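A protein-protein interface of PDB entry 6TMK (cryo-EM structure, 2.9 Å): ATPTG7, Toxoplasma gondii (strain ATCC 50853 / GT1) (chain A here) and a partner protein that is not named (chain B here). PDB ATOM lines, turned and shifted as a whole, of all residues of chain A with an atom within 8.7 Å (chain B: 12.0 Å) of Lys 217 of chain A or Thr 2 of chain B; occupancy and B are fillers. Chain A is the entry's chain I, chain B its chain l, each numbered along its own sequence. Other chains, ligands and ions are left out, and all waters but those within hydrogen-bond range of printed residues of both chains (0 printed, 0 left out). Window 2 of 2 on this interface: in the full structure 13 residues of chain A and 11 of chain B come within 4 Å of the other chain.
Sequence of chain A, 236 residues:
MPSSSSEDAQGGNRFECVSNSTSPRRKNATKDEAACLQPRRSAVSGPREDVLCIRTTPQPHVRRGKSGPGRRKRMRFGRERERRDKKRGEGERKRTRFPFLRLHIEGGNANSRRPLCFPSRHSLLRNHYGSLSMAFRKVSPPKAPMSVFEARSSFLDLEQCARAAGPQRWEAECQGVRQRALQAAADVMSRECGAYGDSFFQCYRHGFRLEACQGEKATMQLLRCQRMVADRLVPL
The side-chain sulfur (SG) of Cys 203 of chain A is disulfide-bonded to the side-chain sulfur (SG) of Cys 213 of chain A (2.0 Å).
Among the printed residues, merely in contact across the chains: Ser 199 of chain A with Pro 5 of chain B (3.5 Å), Lys 217 of chain A with Thr 2 of chain B (3.5 Å), Ala 212 of chain A with Ala 3 of chain B (3.6 Å), Ala 212 of chain A with Pro 5 of chain B (3.6 Å), Ser 199 of chain A with Leu 4 of chain B (3.8 Å) and Gln 221 of chain A with Leu 4 of chain B (3.8 Å).
Lys 217 of chain A touches just one residue of chain B: Thr 2.
Of chain A, only Lys 217 (3.5 Å) comes within 4 Å of Thr 2 of chain B.
No residue of chain B comes within 4 Å of Gly 215 of chain A.
No residue of chain B comes within 4 Å of Glu 216 of chain A.
Ala 218 of chain A touches none of the printed residues of chain B.
Thr 219 of chain A touches none of the printed residues of chain B.
Of chain B, only Leu 4 comes within 4 Å of Gln 221 of chain A.
Printed residues of chain A within 4 Å of Pro 5 of chain B: Ser 199 (3.5 Å) and Ala 212 (3.6 Å).
Printed residues of chain A within 4 Å of Leu 4 of chain B: Ser 199 (3.8 Å) and Gln 221 (3.8 Å).
Of the printed residues of chain B, Ser 199 of chain A touches Leu 4 (3.8 Å) and Pro 5 (3.5 Å).
Glu 211 of chain A touches none of the printed residues of chain B.
Of the 19 printed residues of chain A, 4 touch a printed residue of chain B.
Along chain A the printed residues that touch a printed residue of chain B span positions 199 to 221.
Of the 7 printed residues of chain B, 4 touch a printed residue of chain A.
Printed residues of chain B that touch a printed residue of chain A: Thr 2, Ala 3, Leu 4 and Pro 5.
Hydrophobic or aromatic side chains of chain B within 4 Å of the printed part of chain A: Leu 4 and Pro 5.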
ATOM      1  N   TYR A 196       1.082  -0.608 -12.921  1.00  0.00           N
ATOM      2  CA  TYR A 196       1.919  -0.528 -11.732  1.00  0.00           C
ATOM      3  C   TYR A 196       1.080  -0.581 -10.462  1.00  0.00           C
ATOM      4  O   TYR A 196       1.488  -1.188  -9.465  1.00  0.00           O
ATOM      5  CB  TYR A 196       2.741   0.753 -11.774  1.00  0.00           C
ATOM      6  CG  TYR A 196       3.716   0.816 -12.919  1.00  0.00           C
ATOM      7  CD1 TYR A 196       4.745  -0.100 -13.037  1.00  0.00           C
ATOM      8  CD2 TYR A 196       3.602   1.795 -13.890  1.00  0.00           C
ATOM      9  CE1 TYR A 196       5.632  -0.040 -14.084  1.00  0.00           C
ATOM     10  CE2 TYR A 196       4.483   1.862 -14.937  1.00  0.00           C
ATOM     11  CZ  TYR A 196       5.496   0.945 -15.031  1.00  0.00           C
ATOM     12  OH  TYR A 196       6.372   1.020 -16.083  1.00  0.00           O
ATOM     13  N   SER A 199       0.123  -4.113  -9.952  1.00  0.00           N
ATOM     14  CA  SER A 199       1.271  -4.877  -9.476  1.00  0.00           C
ATOM     15  C   SER A 199       1.506  -4.643  -7.991  1.00  0.00           C
ATOM     16  O   SER A 199       1.789  -5.587  -7.244  1.00  0.00           O
ATOM     17  CB  SER A 199       2.514  -4.511 -10.282  1.00  0.00           C
ATOM     18  OG  SER A 199       2.412  -4.976 -11.611  1.00  0.00           O
ATOM     19  N   PHE A 200       1.401  -3.391  -7.547  1.00  0.00           N
ATOM     20  CA  PHE A 200       1.511  -3.108  -6.123  1.00  0.00           C
ATOM     21  C   PHE A 200       0.408  -3.805  -5.339  1.00  0.00           C
ATOM     22  O   PHE A 200       0.654  -4.351  -4.260  1.00  0.00           O
ATOM     23  CB  PHE A 200       1.458  -1.606  -5.870  1.00  0.00           C
ATOM     24  CG  PHE A 200       1.623  -1.243  -4.432  1.00  0.00           C
ATOM     25  CD1 PHE A 200       2.878  -1.089  -3.891  1.00  0.00           C
ATOM     26  CD2 PHE A 200       0.527  -1.089  -3.611  1.00  0.00           C
ATOM     27  CE1 PHE A 200       3.036  -0.770  -2.575  1.00  0.00           C
ATOM     28  CE2 PHE A 200       0.684  -0.775  -2.290  1.00  0.00           C
ATOM     29  CZ  PHE A 200       1.938  -0.616  -1.772  1.00  0.00           C
ATOM     30  N   CYS A 203       1.330  -7.479  -5.051  1.00  0.00           N
ATOM     31  CA  CYS A 203       2.384  -7.645  -4.061  1.00  0.00           C
ATOM     32  C   CYS A 203       1.846  -7.489  -2.644  1.00  0.00           C
ATOM     33  O   CYS A 203       2.249  -8.219  -1.733  1.00  0.00           O
ATOM     34  CB  CYS A 203       3.492  -6.631  -4.327  1.00  0.00           C
ATOM     35  SG  CYS A 203       4.538  -7.017  -5.730  1.00  0.00           S
ATOM     36  N   LEU A 210       6.908 -11.985  -3.552  1.00  0.00           N
ATOM     37  CA  LEU A 210       7.274 -12.363  -4.903  1.00  0.00           C
ATOM     38  C   LEU A 210       8.581 -11.689  -5.314  1.00  0.00           C
ATOM     39  O   LEU A 210       9.096 -10.795  -4.640  1.00  0.00           O
ATOM     40  CB  LEU A 210       6.162 -11.990  -5.880  1.00  0.00           C
ATOM     41  CG  LEU A 210       4.727 -12.202  -5.407  1.00  0.00           C
ATOM     42  CD1 LEU A 210       3.767 -11.583  -6.382  1.00  0.00           C
ATOM     43  CD2 LEU A 210       4.431 -13.673  -5.255  1.00  0.00           C
ATOM     44  N   GLU A 211       9.116 -12.138  -6.449  1.00  0.00           N
ATOM     45  CA  GLU A 211      10.382 -11.608  -6.944  1.00  0.00           C
ATOM     46  C   GLU A 211      10.250 -10.141  -7.331  1.00  0.00           C
ATOM     47  O   GLU A 211      11.098  -9.314  -6.974  1.00  0.00           O
ATOM     48  CB  GLU A 211      10.864 -12.440  -8.129  1.00  0.00           C
ATOM     49  CG  GLU A 211      11.092 -13.911  -7.800  1.00  0.00           C
ATOM     50  CD  GLU A 211       9.824 -14.734  -7.863  1.00  0.00           C
ATOM     51  OE1 GLU A 211       9.258 -14.874  -8.967  1.00  0.00           O
ATOM     52  OE2 GLU A 211       9.387 -15.232  -6.804  1.00  0.00           O
ATOM     53  N   ALA A 212       9.191  -9.801  -8.063  1.00  0.00           N
ATOM     54  CA  ALA A 212       8.979  -8.436  -8.520  1.00  0.00           C
ATOM     55  C   ALA A 212       8.651  -7.481  -7.387  1.00  0.00           C
ATOM     56  O   ALA A 212       8.706  -6.264  -7.590  1.00  0.00           O
ATOM     57  CB  ALA A 212       7.850  -8.402  -9.541  1.00  0.00           C
ATOM     58  N   CYS A 213       8.316  -7.997  -6.212  1.00  0.00           N
ATOM     59  CA  CYS A 213       8.032  -7.171  -5.053  1.00  0.00           C
ATOM     60  C   CYS A 213       9.274  -6.863  -4.233  1.00  0.00           C
ATOM     61  O   CYS A 213       9.208  -6.031  -3.323  1.00  0.00           O
ATOM     62  CB  CYS A 213       7.004  -7.874  -4.169  1.00  0.00           C
ATOM     63  SG  CYS A 213       5.620  -8.600  -5.072  1.00  0.00           S
ATOM     64  N   GLN A 214      10.393  -7.515  -4.528  1.00  0.00           N
ATOM     65  CA  GLN A 214      11.619  -7.288  -3.780  1.00  0.00           C
ATOM     66  C   GLN A 214      12.186  -5.908  -4.081  1.00  0.00           C
ATOM     67  O   GLN A 214      12.155  -5.440  -5.223  1.00  0.00           O
ATOM     68  CB  GLN A 214      12.646  -8.361  -4.121  1.00  0.00           C
ATOM     69  CG  GLN A 214      12.258  -9.751  -3.657  1.00  0.00           C
ATOM     70  CD  GLN A 214      12.325  -9.907  -2.156  1.00  0.00           C
ATOM     71  OE1 GLN A 214      13.323  -9.559  -1.524  1.00  0.00           O
ATOM     72  NE2 GLN A 214      11.256 -10.434  -1.572  1.00  0.00           N
ATOM     73  N   GLY A 215      12.709  -5.258  -3.047  1.00  0.00           N
ATOM     74  CA  GLY A 215      13.190  -3.899  -3.190  1.00  0.00           C
ATOM     75  C   GLY A 215      12.082  -2.869  -3.042  1.00  0.00           C
ATOM     76  O   GLY A 215      11.106  -3.059  -2.315  1.00  0.00           O
ATOM     77  N   GLU A 216      12.247  -1.757  -3.760  1.00  0.00           N
ATOM     78  CA  GLU A 216      11.312  -0.642  -3.707  1.00  0.00           C
ATOM     79  C   GLU A 216      10.803  -0.258  -5.090  1.00  0.00           C
ATOM     80  O   GLU A 216      10.105   0.755  -5.224  1.00  0.00           O
ATOM     81  CB  GLU A 216      11.972   0.569  -3.042  1.00  0.00           C
ATOM     82  CG  GLU A 216      13.290   0.977  -3.668  1.00  0.00           C
ATOM     83  CD  GLU A 216      13.917   2.172  -2.976  1.00  0.00           C
ATOM     84  OE1 GLU A 216      14.080   2.126  -1.738  1.00  0.00           O
ATOM     85  OE2 GLU A 216      14.247   3.159  -3.667  1.00  0.00           O
ATOM     86  N   LYS A 217      11.133  -1.041  -6.117  1.00  0.00           N
ATOM     87  CA  LYS A 217      10.715  -0.718  -7.473  1.00  0.00           C
ATOM     88  C   LYS A 217       9.201  -0.750  -7.613  1.00  0.00           C
ATOM     89  O   LYS A 217       8.631   0.059  -8.352  1.00  0.00           O
ATOM     90  CB  LYS A 217      11.375  -1.688  -8.446  1.00  0.00           C
ATOM     91  CG  LYS A 217      10.960  -3.119  -8.232  1.00  0.00           C
ATOM     92  CD  LYS A 217      11.833  -4.065  -9.017  1.00  0.00           C
ATOM     93  CE  LYS A 217      11.395  -5.499  -8.818  1.00  0.00           C
ATOM     94  NZ  LYS A 217      12.363  -6.453  -9.409  1.00  0.00           N
ATOM     95  N   ALA A 218       8.533  -1.644  -6.883  1.00  0.00           N
ATOM     96  CA  ALA A 218       7.083  -1.749  -6.981  1.00  0.00           C
ATOM     97  C   ALA A 218       6.405  -0.434  -6.630  1.00  0.00           C
ATOM     98  O   ALA A 218       5.329  -0.128  -7.156  1.00  0.00           O
ATOM     99  CB  ALA A 218       6.583  -2.858  -6.065  1.00  0.00           C
ATOM    100  N   THR A 219       7.014   0.350  -5.747  1.00  0.00           N
ATOM    101  CA  THR A 219       6.491   1.647  -5.344  1.00  0.00           C
ATOM    102  C   THR A 219       7.060   2.776  -6.192  1.00  0.00           C
ATOM    103  O   THR A 219       6.327   3.699  -6.581  1.00  0.00           O
ATOM    104  CB  THR A 219       6.824   1.878  -3.873  1.00  0.00           C
ATOM    105  OG1 THR A 219       6.575   0.676  -3.137  1.00  0.00           O
ATOM    106  CG2 THR A 219       5.998   2.996  -3.298  1.00  0.00           C
ATOM    107  N   MET A 220       8.362   2.720  -6.475  1.00  0.00           N
ATOM    108  CA  MET A 220       9.007   3.801  -7.205  1.00  0.00           C
ATOM    109  C   MET A 220       8.494   3.898  -8.633  1.00  0.00           C
ATOM    110  O   MET A 220       8.373   5.003  -9.165  1.00  0.00           O
ATOM    111  CB  MET A 220      10.520   3.609  -7.197  1.00  0.00           C
ATOM    112  CG  MET A 220      11.168   3.963  -5.877  1.00  0.00           C
ATOM    113  SD  MET A 220      11.173   5.733  -5.539  1.00  0.00           S
ATOM    114  CE  MET A 220      12.710   6.225  -6.315  1.00  0.00           C
ATOM    115  N   GLN A 221       8.173   2.768  -9.264  1.00  0.00           N
ATOM    116  CA  GLN A 221       7.626   2.806 -10.615  1.00  0.00           C
ATOM    117  C   GLN A 221       6.305   3.557 -10.643  1.00  0.00           C
ATOM    118  O   GLN A 221       6.071   4.407 -11.511  1.00  0.00           O
ATOM    119  CB  GLN A 221       7.439   1.381 -11.128  1.00  0.00           C
ATOM    120  CG  GLN A 221       8.725   0.654 -11.444  1.00  0.00           C
ATOM    121  CD  GLN A 221       8.518  -0.837 -11.611  1.00  0.00           C
ATOM    122  OE1 GLN A 221       7.405  -1.340 -11.466  1.00  0.00           O
ATOM    123  NE2 GLN A 221       9.593  -1.555 -11.915  1.00  0.00           N
ATOM    124  N   LEU A 222       5.426   3.250  -9.694  1.00  0.00           N
ATOM    125  CA  LEU A 222       4.132   3.911  -9.624  1.00  0.00           C
ATOM    126  C   LEU A 222       4.293   5.404  -9.370  1.00  0.00           C
ATOM    127  O   LEU A 222       3.664   6.238 -10.038  1.00  0.00           O
ATOM    128  CB  LEU A 222       3.303   3.255  -8.526  1.00  0.00           C
ATOM    129  CG  LEU A 222       1.877   3.725  -8.283  1.00  0.00           C
ATOM    130  CD1 LEU A 222       1.058   3.677  -9.554  1.00  0.00           C
ATOM    131  CD2 LEU A 222       1.269   2.859  -7.224  1.00  0.00           C
ATOM    132  N   LEU A 223       5.135   5.760  -8.399  1.00  0.00           N
ATOM    133  CA  LEU A 223       5.329   7.170  -8.088  1.00  0.00           C
ATOM    134  C   LEU A 223       5.936   7.921  -9.266  1.00  0.00           C
ATOM    135  O   LEU A 223       5.572   9.072  -9.535  1.00  0.00           O
ATOM    136  CB  LEU A 223       6.212   7.303  -6.854  1.00  0.00           C
ATOM    137  CG  LEU A 223       5.651   6.650  -5.595  1.00  0.00           C
ATOM    138  CD1 LEU A 223       6.744   6.473  -4.581  1.00  0.00           C
ATOM    139  CD2 LEU A 223       4.519   7.447  -5.006  1.00  0.00           C
ATOM    140  N   ARG A 224       6.849   7.279  -9.994  1.00  0.00           N
ATOM    141  CA  ARG A 224       7.460   7.907 -11.157  1.00  0.00           C
ATOM    142  C   ARG A 224       6.446   8.104 -12.273  1.00  0.00           C
ATOM    143  O   ARG A 224       6.441   9.143 -12.940  1.00  0.00           O
ATOM    144  CB  ARG A 224       8.637   7.064 -11.629  1.00  0.00           C
ATOM    145  CG  ARG A 224       9.589   7.777 -12.561  1.00  0.00           C
ATOM    146  CD  ARG A 224      10.579   6.804 -13.161  1.00  0.00           C
ATOM    147  NE  ARG A 224      11.284   6.066 -12.113  1.00  0.00           N
ATOM    148  CZ  ARG A 224      11.455   4.747 -12.094  1.00  0.00           C
ATOM    149  NH1 ARG A 224      10.983   3.982 -13.068  1.00  0.00           N
ATOM    150  NH2 ARG A 224      12.106   4.188 -11.088  1.00  0.00           N
ATOM    151  N   THR B   2      13.598  -6.448 -15.646  1.00  0.00           N
ATOM    152  CA  THR B   2      12.830  -7.365 -14.816  1.00  0.00           C
ATOM    153  C   THR B   2      11.348  -7.300 -15.162  1.00  0.00           C
ATOM    154  O   THR B   2      10.871  -6.310 -15.711  1.00  0.00           O
ATOM    155  CB  THR B   2      13.022  -7.062 -13.321  1.00  0.00           C
ATOM    156  OG1 THR B   2      12.413  -8.096 -12.539  1.00  0.00           O
ATOM    157  CG2 THR B   2      12.409  -5.712 -12.962  1.00  0.00           C
ATOM    158  N   ALA B   3      10.626  -8.362 -14.831  1.00  0.00           N
ATOM    159  CA  ALA B   3       9.223  -8.489 -15.188  1.00  0.00           C
ATOM    160  C   ALA B   3       8.316  -7.940 -14.095  1.00  0.00           C
ATOM    161  O   ALA B   3       8.729  -7.712 -12.957  1.00  0.00           O
ATOM    162  CB  ALA B   3       8.866  -9.949 -15.451  1.00  0.00           C
ATOM    163  N   LEU B   4       7.067  -7.728 -14.465  1.00  0.00           N
ATOM    164  CA  LEU B   4       6.025  -7.402 -13.509  1.00  0.00           C
ATOM    165  C   LEU B   4       5.317  -8.666 -13.057  1.00  0.00           C
ATOM    166  O   LEU B   4       5.387  -9.703 -13.723  1.00  0.00           O
ATOM    167  CB  LEU B   4       5.008  -6.460 -14.140  1.00  0.00           C
ATOM    168  CG  LEU B   4       5.435  -5.039 -14.480  1.00  0.00           C
ATOM    169  CD1 LEU B   4       4.216  -4.240 -14.851  1.00  0.00           C
ATOM    170  CD2 LEU B   4       6.178  -4.392 -13.339  1.00  0.00           C
ATOM    171  N   PRO B   5       4.617  -8.619 -11.932  1.00  0.00           N
ATOM    172  CA  PRO B   5       3.799  -9.754 -11.540  1.00  0.00           C
ATOM    173  C   PRO B   5       2.599  -9.881 -12.456  1.00  0.00           C
ATOM    174  O   PRO B   5       2.221  -8.913 -13.132  1.00  0.00           O
ATOM    175  CB  PRO B   5       3.386  -9.414 -10.105  1.00  0.00           C
ATOM    176  CG  PRO B   5       3.471  -7.970 -10.025  1.00  0.00           C
ATOM    177  CD  PRO B   5       4.593  -7.558 -10.916  1.00  0.00           C
ATOM    178  N   PRO B   6       1.973 -11.048 -12.513  1.00  0.00           N
ATOM    179  CA  PRO B   6       0.758 -11.183 -13.299  1.00  0.00           C
ATOM    180  C   PRO B   6      -0.343 -10.298 -12.750  1.00  0.00           C
ATOM    181  O   PRO B   6      -0.331  -9.934 -11.566  1.00  0.00           O
ATOM    182  CB  PRO B   6       0.403 -12.667 -13.144  1.00  0.00           C
ATOM    183  CG  PRO B   6       1.670 -13.319 -12.805  1.00  0.00           C
ATOM    184  CD  PRO B   6       2.410 -12.343 -11.971  1.00  0.00           C
ATOM    185  N   TRP B  49      13.864  -4.241 -32.499  1.00  0.00           N
ATOM    186  CA  TRP B  49      14.689  -4.241 -31.302  1.00  0.00           C
ATOM    187  C   TRP B  49      15.284  -5.614 -31.042  1.00  0.00           C
ATOM    188  O   TRP B  49      16.464  -5.730 -30.697  1.00  0.00           O
ATOM    189  CB  TRP B  49      13.851  -3.781 -30.117  1.00  0.00           C
ATOM    190  CG  TRP B  49      14.626  -3.484 -28.897  1.00  0.00           C
ATOM    191  CD1 TRP B  49      15.187  -2.301 -28.561  1.00  0.00           C
ATOM    192  CD2 TRP B  49      14.916  -4.384 -27.831  1.00  0.00           C
ATOM    193  NE1 TRP B  49      15.818  -2.402 -27.355  1.00  0.00           N
ATOM    194  CE2 TRP B  49      15.664  -3.676 -26.885  1.00  0.00           C
ATOM    195  CE3 TRP B  49      14.618  -5.722 -27.585  1.00  0.00           C
ATOM    196  CZ2 TRP B  49      16.120  -4.258 -25.717  1.00  0.00           C
ATOM    197  CZ3 TRP B  49      15.072  -6.292 -26.433  1.00  0.00           C
ATOM    198  CH2 TRP B  49      15.812  -5.566 -25.511  1.00  0.00           C
ATOM    199  N   LYS B  53      19.221  -6.549 -31.011  1.00  0.00           N
ATOM    200  CA  LYS B  53      19.824  -7.065 -29.789  1.00  0.00           C
ATOM    201  C   LYS B  53      20.517  -8.400 -30.033  1.00  0.00           C
ATOM    202  O   LYS B  53      21.664  -8.607 -29.614  1.00  0.00           O
ATOM    203  CB  LYS B  53      18.736  -7.191 -28.725  1.00  0.00           C
ATOM    204  CG  LYS B  53      19.178  -7.671 -27.380  1.00  0.00           C
ATOM    205  CD  LYS B  53      19.851  -6.579 -26.621  1.00  0.00           C
ATOM    206  CE  LYS B  53      20.417  -7.085 -25.326  1.00  0.00           C
ATOM    207  NZ  LYS B  53      19.340  -7.360 -24.371  1.00  0.00           N
